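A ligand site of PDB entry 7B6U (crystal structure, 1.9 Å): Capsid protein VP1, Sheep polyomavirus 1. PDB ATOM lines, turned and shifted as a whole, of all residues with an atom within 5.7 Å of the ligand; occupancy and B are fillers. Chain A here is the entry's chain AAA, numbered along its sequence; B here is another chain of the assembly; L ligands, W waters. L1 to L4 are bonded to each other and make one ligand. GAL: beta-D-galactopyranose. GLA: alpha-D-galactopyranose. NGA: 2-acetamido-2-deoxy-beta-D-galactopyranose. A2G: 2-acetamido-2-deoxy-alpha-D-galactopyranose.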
ATOM      1  N   GLN A  32     -28.067 -22.952  19.799  1.00  0.00           N
ATOM      2  CA  GLN A  32     -28.756 -22.415  21.005  1.00  0.00           C
ATOM      3  C   GLN A  32     -29.692 -23.494  21.557  1.00  0.00           C
ATOM      4  O   GLN A  32     -30.245 -24.306  20.820  1.00  0.00           O
ATOM      5  CB  GLN A  32     -29.470 -21.096  20.730  1.00  0.00           C
ATOM      6  CG  GLN A  32     -28.546 -19.940  20.398  1.00  0.00           C
ATOM      7  CD  GLN A  32     -28.004 -19.254  21.624  1.00  0.00           C
ATOM      8  OE1 GLN A  32     -27.580 -19.923  22.579  1.00  0.00           O
ATOM      9  NE2 GLN A  32     -28.070 -17.922  21.613  1.00  0.00           N
ATOM     10  N   PHE A  38     -33.592 -18.303  22.088  1.00  0.00           N
ATOM     11  CA  PHE A  38     -32.822 -18.234  20.812  1.00  0.00           C
ATOM     12  C   PHE A  38     -32.933 -19.569  20.085  1.00  0.00           C
ATOM     13  O   PHE A  38     -32.111 -19.816  19.174  1.00  0.00           O
ATOM     14  CB  PHE A  38     -31.399 -17.739  21.078  1.00  0.00           C
ATOM     15  CG  PHE A  38     -31.400 -16.309  21.573  1.00  0.00           C
ATOM     16  CD1 PHE A  38     -31.509 -16.041  22.923  1.00  0.00           C
ATOM     17  CD2 PHE A  38     -31.379 -15.251  20.686  1.00  0.00           C
ATOM     18  CE1 PHE A  38     -31.562 -14.741  23.391  1.00  0.00           C
ATOM     19  CE2 PHE A  38     -31.375 -13.943  21.150  1.00  0.00           C
ATOM     20  CZ  PHE A  38     -31.521 -13.694  22.498  1.00  0.00           C
ATOM     21  N   ASP A  43     -25.652 -19.200  18.783  1.00  0.00           N
ATOM     22  CA  ASP A  43     -25.089 -18.064  19.539  1.00  0.00           C
ATOM     23  C   ASP A  43     -24.192 -17.265  18.581  1.00  0.00           C
ATOM     24  O   ASP A  43     -23.778 -17.763  17.489  1.00  0.00           O
ATOM     25  CB  ASP A  43     -24.342 -18.566  20.774  1.00  0.00           C
ATOM     26  CG  ASP A  43     -24.116 -17.513  21.868  1.00  0.00           C
ATOM     27  OD1 ASP A  43     -24.467 -16.340  21.661  1.00  0.00           O
ATOM     28  OD2 ASP A  43     -23.577 -17.894  22.904  1.00  0.00           O
ATOM     29  N   ASN A  44     -23.856 -16.046  18.979  1.00  0.00           N
ATOM     30  CA  ASN A  44     -23.084 -15.113  18.107  1.00  0.00           C
ATOM     31  C   ASN A  44     -21.712 -15.720  17.798  1.00  0.00           C
ATOM     32  O   ASN A  44     -21.061 -16.173  18.724  1.00  0.00           O
ATOM     33  CB  ASN A  44     -23.090 -13.726  18.749  1.00  0.00           C
ATOM     34  CG  ASN A  44     -24.500 -13.214  18.906  1.00  0.00           C
ATOM     35  OD1 ASN A  44     -25.207 -13.051  17.903  1.00  0.00           O
ATOM     36  ND2 ASN A  44     -24.957 -13.041  20.139  1.00  0.00           N
ATOM     37  N   LYS A  59     -22.276 -23.998  20.890  1.00  0.00           N
ATOM     38  CA  LYS A  59     -23.507 -23.212  20.596  1.00  0.00           C
ATOM     39  C   LYS A  59     -23.264 -22.261  19.412  1.00  0.00           C
ATOM     40  O   LYS A  59     -24.247 -21.665  18.971  1.00  0.00           O
ATOM     41  CB  LYS A  59     -24.031 -22.424  21.795  1.00  0.00           C
ATOM     42  CG  LYS A  59     -24.436 -23.282  22.995  1.00  0.00           C
ATOM     43  CD  LYS A  59     -25.067 -22.459  24.110  1.00  0.00           C
ATOM     44  CE  LYS A  59     -24.095 -21.445  24.666  1.00  0.00           C
ATOM     45  NZ  LYS A  59     -24.452 -20.994  26.037  1.00  0.00           N
ATOM     46  N   GLN A  60     -22.037 -22.086  18.933  1.00  0.00           N
ATOM     47  CA  GLN A  60     -21.743 -21.044  17.904  1.00  0.00           C
ATOM     48  C   GLN A  60     -21.677 -21.676  16.520  1.00  0.00           C
ATOM     49  O   GLN A  60     -21.264 -20.985  15.618  1.00  0.00           O
ATOM     50  CB  GLN A  60     -20.446 -20.288  18.196  1.00  0.00           C
ATOM     51  CG  GLN A  60     -20.610 -19.290  19.336  1.00  0.00           C
ATOM     52  CD  GLN A  60     -19.311 -18.579  19.662  1.00  0.00           C
ATOM     53  OE1 GLN A  60     -18.424 -18.383  18.804  1.00  0.00           O
ATOM     54  NE2 GLN A  60     -19.241 -18.130  20.902  1.00  0.00           N
ATOM     55  N   ALA A 107     -35.156  -6.854  15.782  1.00  0.00           N
ATOM     56  CA  ALA A 107     -33.789  -6.603  16.274  1.00  0.00           C
ATOM     57  C   ALA A 107     -32.744  -6.836  15.182  1.00  0.00           C
ATOM     58  O   ALA A 107     -31.691  -7.411  15.489  1.00  0.00           O
ATOM     59  CB  ALA A 107     -33.488  -7.451  17.480  1.00  0.00           C
ATOM     60  N   PHE A 249     -28.498 -14.235  10.890  1.00  0.00           N
ATOM     61  CA  PHE A 249     -29.146 -13.097  11.574  1.00  0.00           C
ATOM     62  C   PHE A 249     -28.061 -12.110  12.051  1.00  0.00           C
ATOM     63  O   PHE A 249     -27.088 -12.514  12.734  1.00  0.00           O
ATOM     64  CB  PHE A 249     -30.039 -13.648  12.682  1.00  0.00           C
ATOM     65  CG  PHE A 249     -30.490 -12.619  13.680  1.00  0.00           C
ATOM     66  CD1 PHE A 249     -31.083 -11.435  13.266  1.00  0.00           C
ATOM     67  CD2 PHE A 249     -30.355 -12.856  15.036  1.00  0.00           C
ATOM     68  CE1 PHE A 249     -31.497 -10.497  14.195  1.00  0.00           C
ATOM     69  CE2 PHE A 249     -30.815 -11.944  15.969  1.00  0.00           C
ATOM     70  CZ  PHE A 249     -31.393 -10.763  15.547  1.00  0.00           C
ATOM     71  N   GLN A 251     -27.432  -8.557  14.143  1.00  0.00           N
ATOM     72  CA  GLN A 251     -27.933  -7.601  15.158  1.00  0.00           C
ATOM     73  C   GLN A 251     -27.509  -6.180  14.765  1.00  0.00           C
ATOM     74  O   GLN A 251     -26.683  -6.026  13.842  1.00  0.00           O
ATOM     75  CB  GLN A 251     -27.387  -7.956  16.535  1.00  0.00           C
ATOM     76  CG  GLN A 251     -27.876  -9.293  17.084  1.00  0.00           C
ATOM     77  CD  GLN A 251     -27.535  -9.558  18.539  1.00  0.00           C
ATOM     78  OE1 GLN A 251     -28.136 -10.411  19.176  1.00  0.00           O
ATOM     79  NE2 GLN A 251     -26.524  -8.887  19.066  1.00  0.00           N
ATOM     80  N   HIS A 252     -28.028  -5.178  15.458  1.00  0.00           N
ATOM     81  CA  HIS A 252     -27.590  -3.758  15.299  1.00  0.00           C
ATOM     82  C   HIS A 252     -26.084  -3.652  15.581  1.00  0.00           C
ATOM     83  O   HIS A 252     -25.408  -2.990  14.783  1.00  0.00           O
ATOM     84  CB  HIS A 252     -28.438  -2.782  16.154  1.00  0.00           C
ATOM     85  CG  HIS A 252     -29.877  -2.782  15.824  1.00  0.00           C
ATOM     86  ND1 HIS A 252     -30.388  -2.165  14.691  1.00  0.00           N
ATOM     87  CD2 HIS A 252     -30.932  -3.291  16.489  1.00  0.00           C
ATOM     88  CE1 HIS A 252     -31.696  -2.320  14.661  1.00  0.00           C
ATOM     89  NE2 HIS A 252     -32.042  -3.006  15.770  1.00  0.00           N
ATOM     90  N   ASN A 253     -25.547  -4.340  16.583  1.00  0.00           N
ATOM     91  CA  ASN A 253     -24.119  -4.258  16.987  1.00  0.00           C
ATOM     92  C   ASN A 253     -23.269  -5.163  16.083  1.00  0.00           C
ATOM     93  O   ASN A 253     -22.096  -5.318  16.358  1.00  0.00           O
ATOM     94  CB  ASN A 253     -23.904  -4.536  18.482  1.00  0.00           C
ATOM     95  CG  ASN A 253     -24.342  -5.910  18.942  1.00  0.00           C
ATOM     96  OD1 ASN A 253     -24.595  -6.818  18.140  1.00  0.00           O
ATOM     97  ND2 ASN A 253     -24.331  -6.122  20.239  1.00  0.00           N
ATOM     98  N   LYS A 255     -23.297  -8.352  15.541  1.00  0.00           N
ATOM     99  CA  LYS A 255     -23.067  -9.757  15.938  1.00  0.00           C
ATOM    100  C   LYS A 255     -23.938 -10.634  15.023  1.00  0.00           C
ATOM    101  O   LYS A 255     -25.064 -10.236  14.719  1.00  0.00           O
ATOM    102  CB  LYS A 255     -23.402  -9.993  17.413  1.00  0.00           C
ATOM    103  CG  LYS A 255     -22.445  -9.311  18.379  1.00  0.00           C
ATOM    104  CD  LYS A 255     -22.496  -9.903  19.790  1.00  0.00           C
ATOM    105  CE  LYS A 255     -21.703  -9.048  20.755  1.00  0.00           C
ATOM    106  NZ  LYS A 255     -20.297  -9.500  20.787  1.00  0.00           N
ATOM    107  N   ASP B  49     -34.972  -2.938  18.787  1.00  0.00           N
ATOM    108  CA  ASP B  49     -33.562  -3.072  19.233  1.00  0.00           C
ATOM    109  C   ASP B  49     -33.278  -4.424  19.905  1.00  0.00           C
ATOM    110  O   ASP B  49     -32.074  -4.774  20.049  1.00  0.00           O
ATOM    111  CB  ASP B  49     -33.203  -1.918  20.169  1.00  0.00           C
ATOM    112  CG  ASP B  49     -33.372  -0.593  19.449  1.00  0.00           C
ATOM    113  OD1 ASP B  49     -32.935  -0.517  18.265  1.00  0.00           O
ATOM    114  OD2 ASP B  49     -34.015   0.289  20.037  1.00  0.00           O
ATOM    115  N   ASP B  50     -34.315  -5.154  20.314  1.00  0.00           N
ATOM    116  CA  ASP B  50     -34.193  -6.427  21.084  1.00  0.00           C
ATOM    117  C   ASP B  50     -35.428  -7.273  20.751  1.00  0.00           C
ATOM    118  O   ASP B  50     -36.470  -6.692  20.470  1.00  0.00           O
ATOM    119  CB  ASP B  50     -34.058  -6.122  22.598  1.00  0.00           C
ATOM    120  CG  ASP B  50     -33.587  -7.255  23.515  1.00  0.00           C
ATOM    121  OD1 ASP B  50     -34.435  -8.120  23.897  1.00  0.00           O
ATOM    122  OD2 ASP B  50     -32.403  -7.226  23.920  1.00  0.00           O
ATOM    123  N   PHE B  51     -35.316  -8.594  20.818  1.00  0.00           N
ATOM    124  CA  PHE B  51     -36.452  -9.516  20.623  1.00  0.00           C
ATOM    125  C   PHE B  51     -37.433  -9.330  21.775  1.00  0.00           C
ATOM    126  O   PHE B  51     -38.621  -9.607  21.556  1.00  0.00           O
ATOM    127  CB  PHE B  51     -36.033 -10.986  20.618  1.00  0.00           C
ATOM    128  CG  PHE B  51     -35.390 -11.501  19.341  1.00  0.00           C
ATOM    129  CD1 PHE B  51     -35.373 -10.743  18.180  1.00  0.00           C
ATOM    130  CD2 PHE B  51     -34.820 -12.773  19.315  1.00  0.00           C
ATOM    131  CE1 PHE B  51     -34.772 -11.216  17.025  1.00  0.00           C
ATOM    132  CE2 PHE B  51     -34.239 -13.269  18.151  1.00  0.00           C
ATOM    133  CZ  PHE B  51     -34.200 -12.477  17.012  1.00  0.00           C
ATOM    134  N   GLY B  52     -36.936  -8.907  22.954  1.00  0.00           N
ATOM    135  CA  GLY B  52     -37.740  -8.730  24.192  1.00  0.00           C
ATOM    136  C   GLY B  52     -38.742  -7.598  24.071  1.00  0.00           C
ATOM    137  O   GLY B  52     -39.809  -7.712  24.676  1.00  0.00           O
ATOM    138  N   ARG B 148     -41.092 -13.790  20.993  1.00  0.00           N
ATOM    139  CA  ARG B 148     -41.411 -12.700  21.963  1.00  0.00           C
ATOM    140  C   ARG B 148     -42.000 -11.490  21.229  1.00  0.00           C
ATOM    141  O   ARG B 148     -42.421 -10.536  21.918  1.00  0.00           O
ATOM    142  CB  ARG B 148     -40.170 -12.358  22.774  1.00  0.00           C
ATOM    143  CG  ARG B 148     -39.821 -13.380  23.836  1.00  0.00           C
ATOM    144  CD  ARG B 148     -38.624 -12.900  24.597  1.00  0.00           C
ATOM    145  NE  ARG B 148     -37.380 -13.048  23.854  1.00  0.00           N
ATOM    146  CZ  ARG B 148     -36.227 -12.486  24.179  1.00  0.00           C
ATOM    147  NH1 ARG B 148     -36.151 -11.707  25.238  1.00  0.00           N
ATOM    148  NH2 ARG B 148     -35.157 -12.719  23.450  1.00  0.00           N
HETATM  149  C1  GAL L   1     -20.342 -10.620  28.729  1.00  0.00           C
HETATM  150  C2  GAL L   1     -20.948 -11.980  28.468  1.00  0.00           C
HETATM  151  C3  GAL L   1     -19.912 -12.859  27.773  1.00  0.00           C
HETATM  152  C4  GAL L   1     -19.530 -12.215  26.456  1.00  0.00           C
HETATM  153  C5  GAL L   1     -18.897 -10.855  26.808  1.00  0.00           C
HETATM  154  C6  GAL L   1     -18.491 -10.019  25.605  1.00  0.00           C
HETATM  155  O1  GAL L   1     -21.353  -9.779  29.278  1.00  0.00           O
HETATM  156  O2  GAL L   1     -21.361 -12.524  29.721  1.00  0.00           O
HETATM  157  O3  GAL L   1     -20.412 -14.174  27.547  1.00  0.00           O
HETATM  158  O4  GAL L   1     -20.733 -12.092  25.674  1.00  0.00           O
HETATM  159  O5  GAL L   1     -19.832 -10.047  27.527  1.00  0.00           O
HETATM  160  O6  GAL L   1     -17.254 -10.487  25.097  1.00  0.00           O
HETATM  161  C1  GLA L   2     -20.575 -12.619  24.343  1.00  0.00           C
HETATM  162  C2  GLA L   2     -21.662 -11.952  23.489  1.00  0.00           C
HETATM  163  C3  GLA L   2     -23.055 -12.442  23.870  1.00  0.00           C
HETATM  164  C4  GLA L   2     -23.078 -13.961  23.878  1.00  0.00           C
HETATM  165  C5  GLA L   2     -21.974 -14.496  24.791  1.00  0.00           C
HETATM  166  C6  GLA L   2     -21.851 -16.034  24.718  1.00  0.00           C
HETATM  167  O2  GLA L   2     -21.682 -10.557  23.720  1.00  0.00           O
HETATM  168  O3  GLA L   2     -23.966 -11.825  22.958  1.00  0.00           O
HETATM  169  O4  GLA L   2     -22.845 -14.459  22.560  1.00  0.00           O
HETATM  170  O5  GLA L   2     -20.703 -14.045  24.308  1.00  0.00           O
HETATM  171  O6  GLA L   2     -23.063 -16.698  25.052  1.00  0.00           O
HETATM  172  C1  NGA L   3     -25.303 -11.887  23.377  1.00  0.00           C
HETATM  173  C2  NGA L   3     -26.050 -10.691  22.841  1.00  0.00           C
HETATM  174  C3  NGA L   3     -27.544 -10.820  23.029  1.00  0.00           C
HETATM  175  C4  NGA L   3     -27.959 -12.142  22.404  1.00  0.00           C
HETATM  176  C5  NGA L   3     -27.224 -13.258  23.088  1.00  0.00           C
HETATM  177  C6  NGA L   3     -27.565 -14.621  22.517  1.00  0.00           C
HETATM  178  C7  NGA L   3     -25.057  -8.491  22.754  1.00  0.00           C
HETATM  179  C8  NGA L   3     -24.455  -7.371  23.590  1.00  0.00           C
HETATM  180  N2  NGA L   3     -25.531  -9.494  23.459  1.00  0.00           N
HETATM  181  O3  NGA L   3     -28.130  -9.725  22.359  1.00  0.00           O
HETATM  182  O4  NGA L   3     -27.661 -12.087  20.972  1.00  0.00           O
HETATM  183  O5  NGA L   3     -25.817 -13.121  22.931  1.00  0.00           O
HETATM  184  O6  NGA L   3     -26.864 -15.654  23.207  1.00  0.00           O
HETATM  185  O7  NGA L   3     -25.083  -8.495  21.520  1.00  0.00           O
HETATM  186  O5  A2G L   4     -28.842  -8.164  23.930  1.00  0.00           O
HETATM  187  C1  A2G L   4     -29.265  -9.136  22.967  1.00  0.00           C
HETATM  188  C2  A2G L   4     -30.066  -8.563  21.813  1.00  0.00           C
HETATM  189  N2  A2G L   4     -30.302  -9.578  20.755  1.00  0.00           N
HETATM  190  C3  A2G L   4     -29.365  -7.326  21.218  1.00  0.00           C
HETATM  191  O3  A2G L   4     -30.136  -6.663  20.246  1.00  0.00           O
HETATM  192  C4  A2G L   4     -29.035  -6.306  22.302  1.00  0.00           C
HETATM  193  O4  A2G L   4     -30.261  -5.798  22.820  1.00  0.00           O
HETATM  194  C5  A2G L   4     -28.227  -6.964  23.400  1.00  0.00           C
HETATM  195  C6  A2G L   4     -27.948  -6.032  24.560  1.00  0.00           C
HETATM  196  O6  A2G L   4     -27.307  -6.879  25.508  1.00  0.00           O
HETATM  197  C7  A2G L   4     -31.542  -9.969  20.386  1.00  0.00           C
HETATM  198  O7  A2G L   4     -32.576  -9.620  20.936  1.00  0.00           O
HETATM  199  C8  A2G L   4     -31.630 -10.852  19.180  1.00  0.00           C
HETATM  200  O   HOH W   1     -27.527  -4.882  18.972  1.00  0.00           O
HETATM  201  O   HOH W   2     -28.649 -13.680  18.547  1.00  0.00           O
HETATM  202  O   HOH W   3     -18.228 -16.113  23.051  1.00  0.00           O
HETATM  203  O   HOH W   4     -30.176  -3.226  22.994  1.00  0.00           O
HETATM  204  O   HOH W   5     -22.740 -18.992  26.531  1.00  0.00           O
HETATM  205  O   HOH W   6     -33.141 -10.783  23.455  1.00  0.00           O
HETATM  206  O   HOH W   7     -19.921 -12.213  20.465  1.00  0.00           O
HETATM  207  O   HOH W   8     -18.667 -16.134  27.419  1.00  0.00           O
HETATM  208  O   HOH W   9     -20.511 -14.762  21.150  1.00  0.00           O
HETATM  209  O   HOH W  10     -29.924  -6.218  17.425  1.00  0.00           O
HETATM  210  O   HOH W  11     -29.984  -3.261  19.914  1.00  0.00           O
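O3 of A2G L4 sits at hydrogen-bond distance from O of Asp 49 of chain B, 2.7 Å away.
OD2 of Asp 50 of chain B lies within hydrogen-bond range of O4 of A2G L4 (2.8 Å).
OE1 of Gln 251 lies within hydrogen-bond range of O4 of NGA L3 (2.5 Å).
An oxygen (O7) of NGA L3 lies within hydrogen-bond range of the side-chain amide nitrogen of Asn 253.
OD2 of Asp 43 sits at hydrogen-bond distance from O6 of GLA L2 (2.5 Å).
O5 of NGA L3 lies within hydrogen-bond range of ND2 of Asn 44, at 2.9 Å.
The side-chain amide nitrogen of Gln 32 lies within hydrogen-bond range of an oxygen (O6) of NGA L3.
NZ of Lys 255 lies close to O2 of GLA L2 (3.4 Å).
The backbone NH (N) of Phe 51 of chain B lies within hydrogen-bond range of an oxygen (O7) of A2G L4, 2.9 Å away.
The side-chain amide oxygen (OE1) of Gln 60 lies close to the backbone carbonyl oxygen (O) of Asn 44.
The side-chain amide nitrogen (NE2) of Gln 251 sits at hydrogen-bond distance from the side-chain amide oxygen (OD1) of Asn 253 (3.0 Å).
N of Gly 52 of chain B is in hydrogen-bond range of OD1 of Asp 50 of chain B (2.8 Å).
The side-chain amide oxygen (OD1) of Asn 253 sits close to the backbone NH (N) of Lys 255 (3.3 Å).
O of Lys 59 sits at hydrogen-bond distance from N of Asp 43 (2.8 Å).
Merely in contact with the ligand: Phe 249 and Phe 38.
Hydrophobic or aromatic side chains that line the ligand: Phe 38, Phe 249 and Phe 51 of chain B.
Within 4 Å of the ligand: Gln 32, Phe 38, Asp 43, Asn 44, Phe 249, Gln 251, Asn 253, Lys 255, Asp 49 of chain B, Asp 50 of chain B and Phe 51 of chain B.
Water W9 lies within hydrogen-bond range of an oxygen (O4) of GLA L2 and the backbone carbonyl oxygen of Asn 44.
Water W5 lies within hydrogen-bond range of the side-chain amino group of Lys 59 (2.7 Å) and an oxygen (O6) of GLA L2 (2.7 Å).
Water W6 lies within hydrogen-bond range of the guanidinium group (NH2) of Arg 148 of chain B (2.8 Å), an oxygen (O7) of A2G L4 (2.8 Å) and the side-chain carboxylate (OD1) of Asp 50 of chain B (3.0 Å).
Water W10 lies within hydrogen-bond range of an oxygen (O3) of A2G L4, the backbone carbonyl oxygen of Ala 107 and the backbone NH of His 252.
Water W1 bridges N of Asn 253 and O3 of A2G L4.
Water W3 lies within hydrogen-bond range of NE2 of Gln 60 and O5 of GLA L2.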
